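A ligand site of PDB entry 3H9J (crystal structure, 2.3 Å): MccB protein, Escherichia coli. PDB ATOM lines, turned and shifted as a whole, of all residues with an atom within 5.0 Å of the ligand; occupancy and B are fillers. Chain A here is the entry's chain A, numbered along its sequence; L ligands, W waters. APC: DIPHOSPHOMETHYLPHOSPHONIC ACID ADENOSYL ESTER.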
ATOM      1  N   GLY A 125      -1.572 -15.728 -23.499  1.00  0.00           N
ATOM      2  CA  GLY A 125      -0.840 -16.961 -23.829  1.00  0.00           C
ATOM      3  C   GLY A 125      -1.386 -17.545 -25.111  1.00  0.00           C
ATOM      4  O   GLY A 125      -2.522 -17.997 -25.158  1.00  0.00           O
ATOM      5  N   CYS A 126      -0.564 -17.503 -26.172  1.00  0.00           N
ATOM      6  CA  CYS A 126      -0.994 -17.961 -27.492  1.00  0.00           C
ATOM      7  C   CYS A 126      -0.251 -19.204 -27.978  1.00  0.00           C
ATOM      8  O   CYS A 126      -0.079 -19.404 -29.190  1.00  0.00           O
ATOM      9  CB  CYS A 126      -0.888 -16.826 -28.532  1.00  0.00           C
ATOM     10  SG  CYS A 126      -2.060 -15.449 -28.226  1.00  0.00           S
ATOM     11  N   GLY A 127       0.165 -20.050 -27.044  1.00  0.00           N
ATOM     12  CA  GLY A 127       0.776 -21.317 -27.390  1.00  0.00           C
ATOM     13  C   GLY A 127      -0.275 -22.360 -27.655  1.00  0.00           C
ATOM     14  O   GLY A 127      -1.340 -22.043 -28.216  1.00  0.00           O
ATOM     15  N   GLY A 128       0.002 -23.594 -27.253  1.00  0.00           N
ATOM     16  CA  GLY A 128      -0.859 -24.757 -27.530  1.00  0.00           C
ATOM     17  C   GLY A 128      -2.282 -24.622 -27.008  1.00  0.00           C
ATOM     18  O   GLY A 128      -3.221 -24.946 -27.716  1.00  0.00           O
ATOM     19  N   ILE A 129      -2.432 -24.139 -25.779  1.00  0.00           N
ATOM     20  CA  ILE A 129      -3.756 -23.946 -25.193  1.00  0.00           C
ATOM     21  C   ILE A 129      -4.528 -22.801 -25.862  1.00  0.00           C
ATOM     22  O   ILE A 129      -5.684 -22.958 -26.235  1.00  0.00           O
ATOM     23  CB  ILE A 129      -3.680 -23.720 -23.671  1.00  0.00           C
ATOM     24  CG1 ILE A 129      -3.089 -24.959 -22.961  1.00  0.00           C
ATOM     25  CG2 ILE A 129      -5.048 -23.292 -23.084  1.00  0.00           C
ATOM     26  CD1 ILE A 129      -4.051 -26.138 -22.828  1.00  0.00           C
ATOM     27  N   ILE A 148      -2.859 -12.100 -26.745  1.00  0.00           N
ATOM     28  CA  ILE A 148      -1.701 -11.533 -26.053  1.00  0.00           C
ATOM     29  C   ILE A 148      -0.579 -12.553 -25.932  1.00  0.00           C
ATOM     30  O   ILE A 148      -0.782 -13.676 -25.465  1.00  0.00           O
ATOM     31  CB  ILE A 148      -2.104 -10.921 -24.694  1.00  0.00           C
ATOM     32  CG1 ILE A 148      -3.232  -9.896 -24.904  1.00  0.00           C
ATOM     33  CG2 ILE A 148      -0.877 -10.302 -23.994  1.00  0.00           C
ATOM     34  CD1 ILE A 148      -3.974  -9.465 -23.665  1.00  0.00           C
ATOM     35  N   ASP A 149       0.614 -12.139 -26.397  1.00  0.00           N
ATOM     36  CA  ASP A 149       1.802 -12.974 -26.518  1.00  0.00           C
ATOM     37  C   ASP A 149       2.903 -12.137 -27.168  1.00  0.00           C
ATOM     38  O   ASP A 149       2.615 -11.291 -28.018  1.00  0.00           O
ATOM     39  CB  ASP A 149       1.522 -14.207 -27.393  1.00  0.00           C
ATOM     40  CG  ASP A 149       2.446 -15.372 -27.099  1.00  0.00           C
ATOM     41  OD1 ASP A 149       3.680 -15.209 -27.203  1.00  0.00           O
ATOM     42  OD2 ASP A 149       1.938 -16.469 -26.783  1.00  0.00           O
ATOM     43  N   ASN A 150       4.162 -12.362 -26.769  1.00  0.00           N
ATOM     44  CA  ASN A 150       5.297 -11.646 -27.367  1.00  0.00           C
ATOM     45  C   ASN A 150       6.224 -12.567 -28.173  1.00  0.00           C
ATOM     46  O   ASN A 150       7.051 -12.097 -28.940  1.00  0.00           O
ATOM     47  CB  ASN A 150       6.095 -10.905 -26.281  1.00  0.00           C
ATOM     48  CG  ASN A 150       6.818  -9.633 -26.808  1.00  0.00           C
ATOM     49  OD1 ASN A 150       6.249  -8.825 -27.548  1.00  0.00           O
ATOM     50  ND2 ASN A 150       8.063  -9.455 -26.389  1.00  0.00           N
ATOM     51  N   ASP A 151       6.041 -13.887 -28.013  1.00  0.00           N
ATOM     52  CA  ASP A 151       6.873 -14.877 -28.707  1.00  0.00           C
ATOM     53  C   ASP A 151       6.606 -15.031 -30.214  1.00  0.00           C
ATOM     54  O   ASP A 151       5.572 -14.614 -30.714  1.00  0.00           O
ATOM     55  CB  ASP A 151       6.748 -16.244 -28.033  1.00  0.00           C
ATOM     56  CG  ASP A 151       7.507 -16.323 -26.712  1.00  0.00           C
ATOM     57  OD1 ASP A 151       7.119 -15.606 -25.754  1.00  0.00           O
ATOM     58  OD2 ASP A 151       8.473 -17.117 -26.651  1.00  0.00           O
ATOM     59  N   ASN A 157       6.463 -25.970 -32.411  1.00  0.00           N
ATOM     60  CA  ASN A 157       5.127 -25.545 -32.005  1.00  0.00           C
ATOM     61  C   ASN A 157       4.077 -26.343 -32.755  1.00  0.00           C
ATOM     62  O   ASN A 157       2.943 -26.500 -32.272  1.00  0.00           O
ATOM     63  CB  ASN A 157       4.914 -24.050 -32.330  1.00  0.00           C
ATOM     64  CG  ASN A 157       5.811 -23.109 -31.515  1.00  0.00           C
ATOM     65  OD1 ASN A 157       5.912 -21.923 -31.843  1.00  0.00           O
ATOM     66  ND2 ASN A 157       6.456 -23.628 -30.459  1.00  0.00           N
ATOM     67  N   ARG A 160       1.283 -28.994 -31.330  1.00  0.00           N
ATOM     68  CA  ARG A 160       0.068 -28.676 -30.572  1.00  0.00           C
ATOM     69  C   ARG A 160      -0.707 -27.508 -31.187  1.00  0.00           C
ATOM     70  O   ARG A 160      -1.948 -27.455 -31.112  1.00  0.00           O
ATOM     71  CB  ARG A 160       0.424 -28.263 -29.135  1.00  0.00           C
ATOM     72  CG  ARG A 160       0.946 -29.341 -28.204  1.00  0.00           C
ATOM     73  CD  ARG A 160       2.448 -29.275 -28.040  1.00  0.00           C
ATOM     74  NE  ARG A 160       2.972 -27.970 -27.598  1.00  0.00           N
ATOM     75  CZ  ARG A 160       4.157 -27.494 -27.985  1.00  0.00           C
ATOM     76  NH1 ARG A 160       4.933 -28.195 -28.806  1.00  0.00           N
ATOM     77  NH2 ARG A 160       4.581 -26.318 -27.558  1.00  0.00           N
ATOM     78  N   GLN A 161       0.039 -26.550 -31.742  1.00  0.00           N
ATOM     79  CA  GLN A 161      -0.466 -25.236 -32.161  1.00  0.00           C
ATOM     80  C   GLN A 161      -1.047 -25.305 -33.564  1.00  0.00           C
ATOM     81  O   GLN A 161      -0.407 -24.997 -34.554  1.00  0.00           O
ATOM     82  CB  GLN A 161       0.633 -24.174 -31.963  1.00  0.00           C
ATOM     83  CG  GLN A 161       0.957 -23.985 -30.458  1.00  0.00           C
ATOM     84  CD  GLN A 161       2.280 -23.290 -30.123  1.00  0.00           C
ATOM     85  OE1 GLN A 161       2.612 -22.247 -30.693  1.00  0.00           O
ATOM     86  NE2 GLN A 161       3.020 -23.859 -29.180  1.00  0.00           N
ATOM     87  N   LYS A 173       3.160 -15.084 -33.051  1.00  0.00           N
ATOM     88  CA  LYS A 173       2.043 -15.996 -32.827  1.00  0.00           C
ATOM     89  C   LYS A 173       0.697 -15.281 -32.981  1.00  0.00           C
ATOM     90  O   LYS A 173      -0.175 -15.752 -33.703  1.00  0.00           O
ATOM     91  CB  LYS A 173       2.134 -16.669 -31.443  1.00  0.00           C
ATOM     92  CG  LYS A 173       3.370 -17.557 -31.291  1.00  0.00           C
ATOM     93  CD  LYS A 173       3.373 -18.305 -29.975  1.00  0.00           C
ATOM     94  CE  LYS A 173       4.684 -19.037 -29.783  1.00  0.00           C
ATOM     95  NZ  LYS A 173       4.607 -19.946 -28.611  1.00  0.00           N
ATOM     96  N   LEU A 195       2.965  -8.224 -25.838  1.00  0.00           N
ATOM     97  CA  LEU A 195       3.303  -8.065 -24.429  1.00  0.00           C
ATOM     98  C   LEU A 195       3.889  -9.349 -23.862  1.00  0.00           C
ATOM     99  O   LEU A 195       3.364 -10.449 -24.089  1.00  0.00           O
ATOM    100  CB  LEU A 195       2.047  -7.671 -23.642  1.00  0.00           C
ATOM    101  CG  LEU A 195       2.142  -7.332 -22.149  1.00  0.00           C
ATOM    102  CD1 LEU A 195       2.536  -5.874 -21.966  1.00  0.00           C
ATOM    103  CD2 LEU A 195       0.821  -7.593 -21.484  1.00  0.00           C
ATOM    104  N   ASN A 196       4.979  -9.199 -23.132  1.00  0.00           N
ATOM    105  CA  ASN A 196       5.460 -10.285 -22.283  1.00  0.00           C
ATOM    106  C   ASN A 196       5.438  -9.843 -20.829  1.00  0.00           C
ATOM    107  O   ASN A 196       5.931  -8.775 -20.480  1.00  0.00           O
ATOM    108  CB  ASN A 196       6.845 -10.798 -22.697  1.00  0.00           C
ATOM    109  CG  ASN A 196       7.020 -12.302 -22.433  1.00  0.00           C
ATOM    110  OD1 ASN A 196       7.570 -12.693 -21.411  1.00  0.00           O
ATOM    111  ND2 ASN A 196       6.524 -13.143 -23.365  1.00  0.00           N
ATOM    112  N   ILE A 197       4.825 -10.675 -19.982  1.00  0.00           N
ATOM    113  CA  ILE A 197       4.620 -10.333 -18.579  1.00  0.00           C
ATOM    114  C   ILE A 197       5.845 -10.696 -17.731  1.00  0.00           C
ATOM    115  O   ILE A 197       6.057 -11.860 -17.342  1.00  0.00           O
ATOM    116  CB  ILE A 197       3.278 -10.911 -18.046  1.00  0.00           C
ATOM    117  CG1 ILE A 197       2.128 -10.298 -18.851  1.00  0.00           C
ATOM    118  CG2 ILE A 197       3.115 -10.622 -16.551  1.00  0.00           C
ATOM    119  CD1 ILE A 197       0.862 -11.081 -18.823  1.00  0.00           C
ATOM    120  N   ASN A 198       6.673  -9.677 -17.487  1.00  0.00           N
ATOM    121  CA  ASN A 198       7.912  -9.797 -16.739  1.00  0.00           C
ATOM    122  C   ASN A 198       7.674  -9.600 -15.247  1.00  0.00           C
ATOM    123  O   ASN A 198       8.354 -10.205 -14.417  1.00  0.00           O
ATOM    124  CB  ASN A 198       8.936  -8.756 -17.221  1.00  0.00           C
ATOM    125  CG  ASN A 198       9.035  -8.676 -18.736  1.00  0.00           C
ATOM    126  OD1 ASN A 198       9.035  -9.695 -19.429  1.00  0.00           O
ATOM    127  ND2 ASN A 198       9.145  -7.447 -19.245  1.00  0.00           N
ATOM    128  N   SER A 215      -3.199 -19.164 -20.112  1.00  0.00           N
ATOM    129  CA  SER A 215      -2.369 -20.366 -20.254  1.00  0.00           C
ATOM    130  C   SER A 215      -0.842 -20.100 -20.238  1.00  0.00           C
ATOM    131  O   SER A 215      -0.049 -21.039 -20.152  1.00  0.00           O
ATOM    132  CB  SER A 215      -2.795 -21.191 -21.460  1.00  0.00           C
ATOM    133  OG  SER A 215      -2.787 -20.428 -22.643  1.00  0.00           O
ATOM    134  N   ALA A 216      -0.444 -18.844 -20.324  1.00  0.00           N
ATOM    135  CA  ALA A 216       0.966 -18.495 -20.133  1.00  0.00           C
ATOM    136  C   ALA A 216       1.420 -19.017 -18.768  1.00  0.00           C
ATOM    137  O   ALA A 216       0.702 -18.874 -17.780  1.00  0.00           O
ATOM    138  CB  ALA A 216       1.168 -16.973 -20.241  1.00  0.00           C
ATOM    139  N   ASP A 217       2.585 -19.666 -18.710  1.00  0.00           N
ATOM    140  CA  ASP A 217       3.044 -20.280 -17.458  1.00  0.00           C
ATOM    141  C   ASP A 217       4.484 -19.911 -17.104  1.00  0.00           C
ATOM    142  O   ASP A 217       5.147 -20.630 -16.346  1.00  0.00           O
ATOM    143  CB  ASP A 217       2.853 -21.822 -17.500  1.00  0.00           C
ATOM    144  N   HIS A 218       4.949 -18.783 -17.634  1.00  0.00           N
ATOM    145  CA  HIS A 218       6.271 -18.241 -17.315  1.00  0.00           C
ATOM    146  C   HIS A 218       6.233 -16.764 -16.878  1.00  0.00           C
ATOM    147  O   HIS A 218       5.632 -15.953 -17.558  1.00  0.00           O
ATOM    148  CB  HIS A 218       7.211 -18.434 -18.500  1.00  0.00           C
ATOM    149  CG  HIS A 218       7.811 -19.798 -18.586  1.00  0.00           C
ATOM    150  ND1 HIS A 218       7.082 -20.909 -18.959  1.00  0.00           N
ATOM    151  CD2 HIS A 218       9.072 -20.239 -18.339  1.00  0.00           C
ATOM    152  CE1 HIS A 218       7.874 -21.978 -18.936  1.00  0.00           C
ATOM    153  NE2 HIS A 218       9.073 -21.593 -18.560  1.00  0.00           N
ATOM    154  N   PRO A 219       6.875 -16.424 -15.740  1.00  0.00           N
ATOM    155  CA  PRO A 219       7.641 -17.303 -14.834  1.00  0.00           C
ATOM    156  C   PRO A 219       6.738 -18.183 -13.973  1.00  0.00           C
ATOM    157  O   PRO A 219       5.529 -18.237 -14.198  1.00  0.00           O
ATOM    158  CB  PRO A 219       8.419 -16.302 -13.965  1.00  0.00           C
ATOM    159  CG  PRO A 219       7.557 -15.097 -13.933  1.00  0.00           C
ATOM    160  CD  PRO A 219       6.884 -15.021 -15.273  1.00  0.00           C
ATOM    161  N   LEU A 222       3.524 -16.649 -12.376  1.00  0.00           N
ATOM    162  CA  LEU A 222       2.708 -15.826 -13.274  1.00  0.00           C
ATOM    163  C   LEU A 222       1.227 -15.861 -12.905  1.00  0.00           C
ATOM    164  O   LEU A 222       0.550 -14.829 -12.873  1.00  0.00           O
ATOM    165  CB  LEU A 222       2.896 -16.274 -14.735  1.00  0.00           C
ATOM    166  CG  LEU A 222       2.025 -15.601 -15.811  1.00  0.00           C
ATOM    167  CD1 LEU A 222       2.212 -14.101 -15.866  1.00  0.00           C
ATOM    168  CD2 LEU A 222       2.319 -16.188 -17.150  1.00  0.00           C
ATOM    169  N   TYR A 242      -1.469 -27.991 -18.315  1.00  0.00           N
ATOM    170  CA  TYR A 242      -1.119 -29.372 -18.082  1.00  0.00           C
ATOM    171  C   TYR A 242       0.069 -29.431 -17.147  1.00  0.00           C
ATOM    172  O   TYR A 242       0.870 -28.489 -17.065  1.00  0.00           O
ATOM    173  CB  TYR A 242      -0.752 -30.086 -19.392  1.00  0.00           C
ATOM    174  CG  TYR A 242      -0.012 -29.211 -20.362  1.00  0.00           C
ATOM    175  CD1 TYR A 242       1.380 -29.063 -20.278  1.00  0.00           C
ATOM    176  CD2 TYR A 242      -0.697 -28.503 -21.355  1.00  0.00           C
ATOM    177  CE1 TYR A 242       2.060 -28.231 -21.160  1.00  0.00           C
ATOM    178  CE2 TYR A 242      -0.018 -27.670 -22.237  1.00  0.00           C
ATOM    179  CZ  TYR A 242       1.363 -27.546 -22.133  1.00  0.00           C
ATOM    180  OH  TYR A 242       2.035 -26.717 -23.019  1.00  0.00           O
ATOM    181  N   THR A 293       5.181 -32.230 -23.100  1.00  0.00           N
ATOM    182  CA  THR A 293       4.015 -31.796 -23.891  1.00  0.00           C
ATOM    183  C   THR A 293       3.550 -32.918 -24.802  1.00  0.00           C
ATOM    184  O   THR A 293       4.354 -33.699 -25.332  1.00  0.00           O
ATOM    185  CB  THR A 293       4.329 -30.564 -24.784  1.00  0.00           C
ATOM    186  OG1 THR A 293       5.432 -30.868 -25.649  1.00  0.00           O
ATOM    187  CG2 THR A 293       4.684 -29.352 -23.938  1.00  0.00           C
HETATM  188  PG  APC L   1       3.279 -23.475 -25.336  1.00  0.00           P
HETATM  189  O1G APC L   1       1.830 -23.159 -25.132  1.00  0.00           O
HETATM  190  O2G APC L   1       3.979 -22.661 -26.410  1.00  0.00           O
HETATM  191  O3G APC L   1       3.569 -24.969 -25.357  1.00  0.00           O
HETATM  192  PB  APC L   1       5.544 -23.130 -23.676  1.00  0.00           P
HETATM  193  O1B APC L   1       6.331 -22.426 -24.766  1.00  0.00           O
HETATM  194  O2B APC L   1       5.754 -24.620 -23.495  1.00  0.00           O
HETATM  195  O3B APC L   1       3.976 -22.945 -23.984  1.00  0.00           O
HETATM  196  PA  APC L   1       4.393 -21.523 -21.404  1.00  0.00           P
HETATM  197  O1A APC L   1       4.810 -20.758 -20.169  1.00  0.00           O
HETATM  198  O2A APC L   1       3.343 -22.590 -21.209  1.00  0.00           O
HETATM  199  C3A APC L   1       5.891 -22.300 -22.100  1.00  0.00           C
HETATM  200  O5' APC L   1       3.852 -20.439 -22.473  1.00  0.00           O
HETATM  201  C5' APC L   1       2.668 -20.619 -23.278  1.00  0.00           C
HETATM  202  C4' APC L   1       2.483 -19.459 -24.252  1.00  0.00           C
HETATM  203  O4' APC L   1       2.309 -18.263 -23.486  1.00  0.00           O
HETATM  204  C3' APC L   1       3.669 -19.224 -25.181  1.00  0.00           C
HETATM  205  O3' APC L   1       3.214 -18.889 -26.508  1.00  0.00           O
HETATM  206  C2' APC L   1       4.425 -18.049 -24.585  1.00  0.00           C
HETATM  207  O2' APC L   1       4.959 -17.164 -25.570  1.00  0.00           O
HETATM  208  C1' APC L   1       3.352 -17.336 -23.772  1.00  0.00           C
HETATM  209  N9  APC L   1       3.897 -16.786 -22.503  1.00  0.00           N
HETATM  210  C8  APC L   1       4.514 -17.451 -21.514  1.00  0.00           C
HETATM  211  N7  APC L   1       4.826 -16.574 -20.546  1.00  0.00           N
HETATM  212  C5  APC L   1       4.402 -15.348 -20.941  1.00  0.00           C
HETATM  213  C6  APC L   1       4.423 -14.072 -20.397  1.00  0.00           C
HETATM  214  N6  APC L   1       4.984 -13.844 -19.183  1.00  0.00           N
HETATM  215  N1  APC L   1       3.879 -13.036 -21.072  1.00  0.00           N
HETATM  216  C2  APC L   1       3.303 -13.214 -22.281  1.00  0.00           C
HETATM  217  N3  APC L   1       3.268 -14.425 -22.838  1.00  0.00           N
HETATM  218  C4  APC L   1       3.808 -15.506 -22.182  1.00  0.00           C
HETATM  219  O   HOH W   1       0.278 -24.074 -20.815  1.00  0.00           O
HETATM  220  O   HOH W   2       1.091 -26.999 -25.534  1.00  0.00           O
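Gly 125 touches the ligand.
Cys 126 touches the ligand.
O of Leu 195 touches C2 of the ligand, 3.3 Å away.
Asn 196 touches the ligand.
Ser 215 touches the ligand.
CB of Ala 216 touches N9 of the ligand (3.5 Å).
17 residues have an atom within 4 Å of the ligand: Gly 125, Cys 126, Gly 127, Gly 128, Asp 149, Asp 151, Arg 160, Gln 161, Lys 173, Leu 195, Asn 196, Ile 197, Ser 215, Ala 216, Asp 217, His 218 and Tyr 242.
The nearest printed residue that does not touch the ligand is Leu 222 (4.1 Å).
The backbone NH (N) of His 218 sits at hydrogen-bond distance from an oxygen (O1A) of the ligand, 3.2 Å away.
A nitrogen (N6) of the ligand lies within hydrogen-bond range of the backbone carbonyl oxygen (O) of His 218 (2.7 Å).
A ring nitrogen (ND1) of His 218 is in hydrogen-bond range of an oxygen (O1A) of the ligand.
The side-chain carboxylate (OD1) of Asp 151 sits at hydrogen-bond distance from an oxygen (O2') of the ligand (2.7 Å).
The side-chain amino group (NZ) of Lys 173 is in salt-bridge range of an oxygen (O2G) of the ligand (3.6 Å).
The side-chain carboxylate (OD2) of Asp 149 sits at hydrogen-bond distance from an oxygen (O3') of the ligand, 2.7 Å away.
N1 of the ligand is in hydrogen-bond range of N of Ile 197 (2.8 Å).
N6 of the ligand is in hydrogen-bond range of O of Ile 197, at 2.9 Å.
The guanidinium group (NH2) of Arg 160 lies within salt-bridge range of an oxygen (O3G) of the ligand (2.8 Å).
N of Gly 128 is in hydrogen-bond range of O1G of the ligand.
The backbone NH (N) of Asp 217 sits at hydrogen-bond distance from an oxygen (O1A) of the ligand, at 2.9 Å.
The backbone NH of Gly 127 is in hydrogen-bond range of an oxygen (O3') of the ligand (3.3 Å).
An oxygen (O2G) of the ligand lies within hydrogen-bond range of the side-chain amide nitrogen (NE2) of Gln 161, 3.2 Å away.
An oxygen (O3G) of the ligand sits at hydrogen-bond distance from the side-chain hydroxyl (OH) of Tyr 242, 3.3 Å away.
Water W2 lies within hydrogen-bond range of the side-chain hydroxyl (OH) of Tyr 242 (2.7 Å), the guanidinium group (NE) of Arg 160 (3.0 Å) and an oxygen (O3G) of the ligand (3.2 Å).
Water W1 bridges the backbone carbonyl oxygen (O) of Ser 215 (3.1 Å) and an oxygen (O2A) of the ligand (3.4 Å).
The backbone NH of Lys 173 is in hydrogen-bond range of the backbone carbonyl oxygen of Asp 151, 3.4 Å away.
The backbone NH of Asp 151 sits at hydrogen-bond distance from the side-chain carboxylate of Asp 149 (2.8 Å).
The side-chain carboxylate (OD1) of Asp 151 is in hydrogen-bond range of the side-chain amide nitrogen (ND2) of Asn 196.
The backbone NH of Cys 126 sits at hydrogen-bond distance from the side-chain carboxylate of Asp 149 (2.8 Å).
NH2 of Arg 160 sits close to NE2 of Gln 161, at 3.3 Å.
O of Leu 195 lies within hydrogen-bond range of N of Asn 150, at 3.4 Å.
N of Gly 125 sits at hydrogen-bond distance from O of Ile 148 (2.9 Å).
O of Ile 148 lies within hydrogen-bond range of SG of Cys 126 (3.5 Å).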
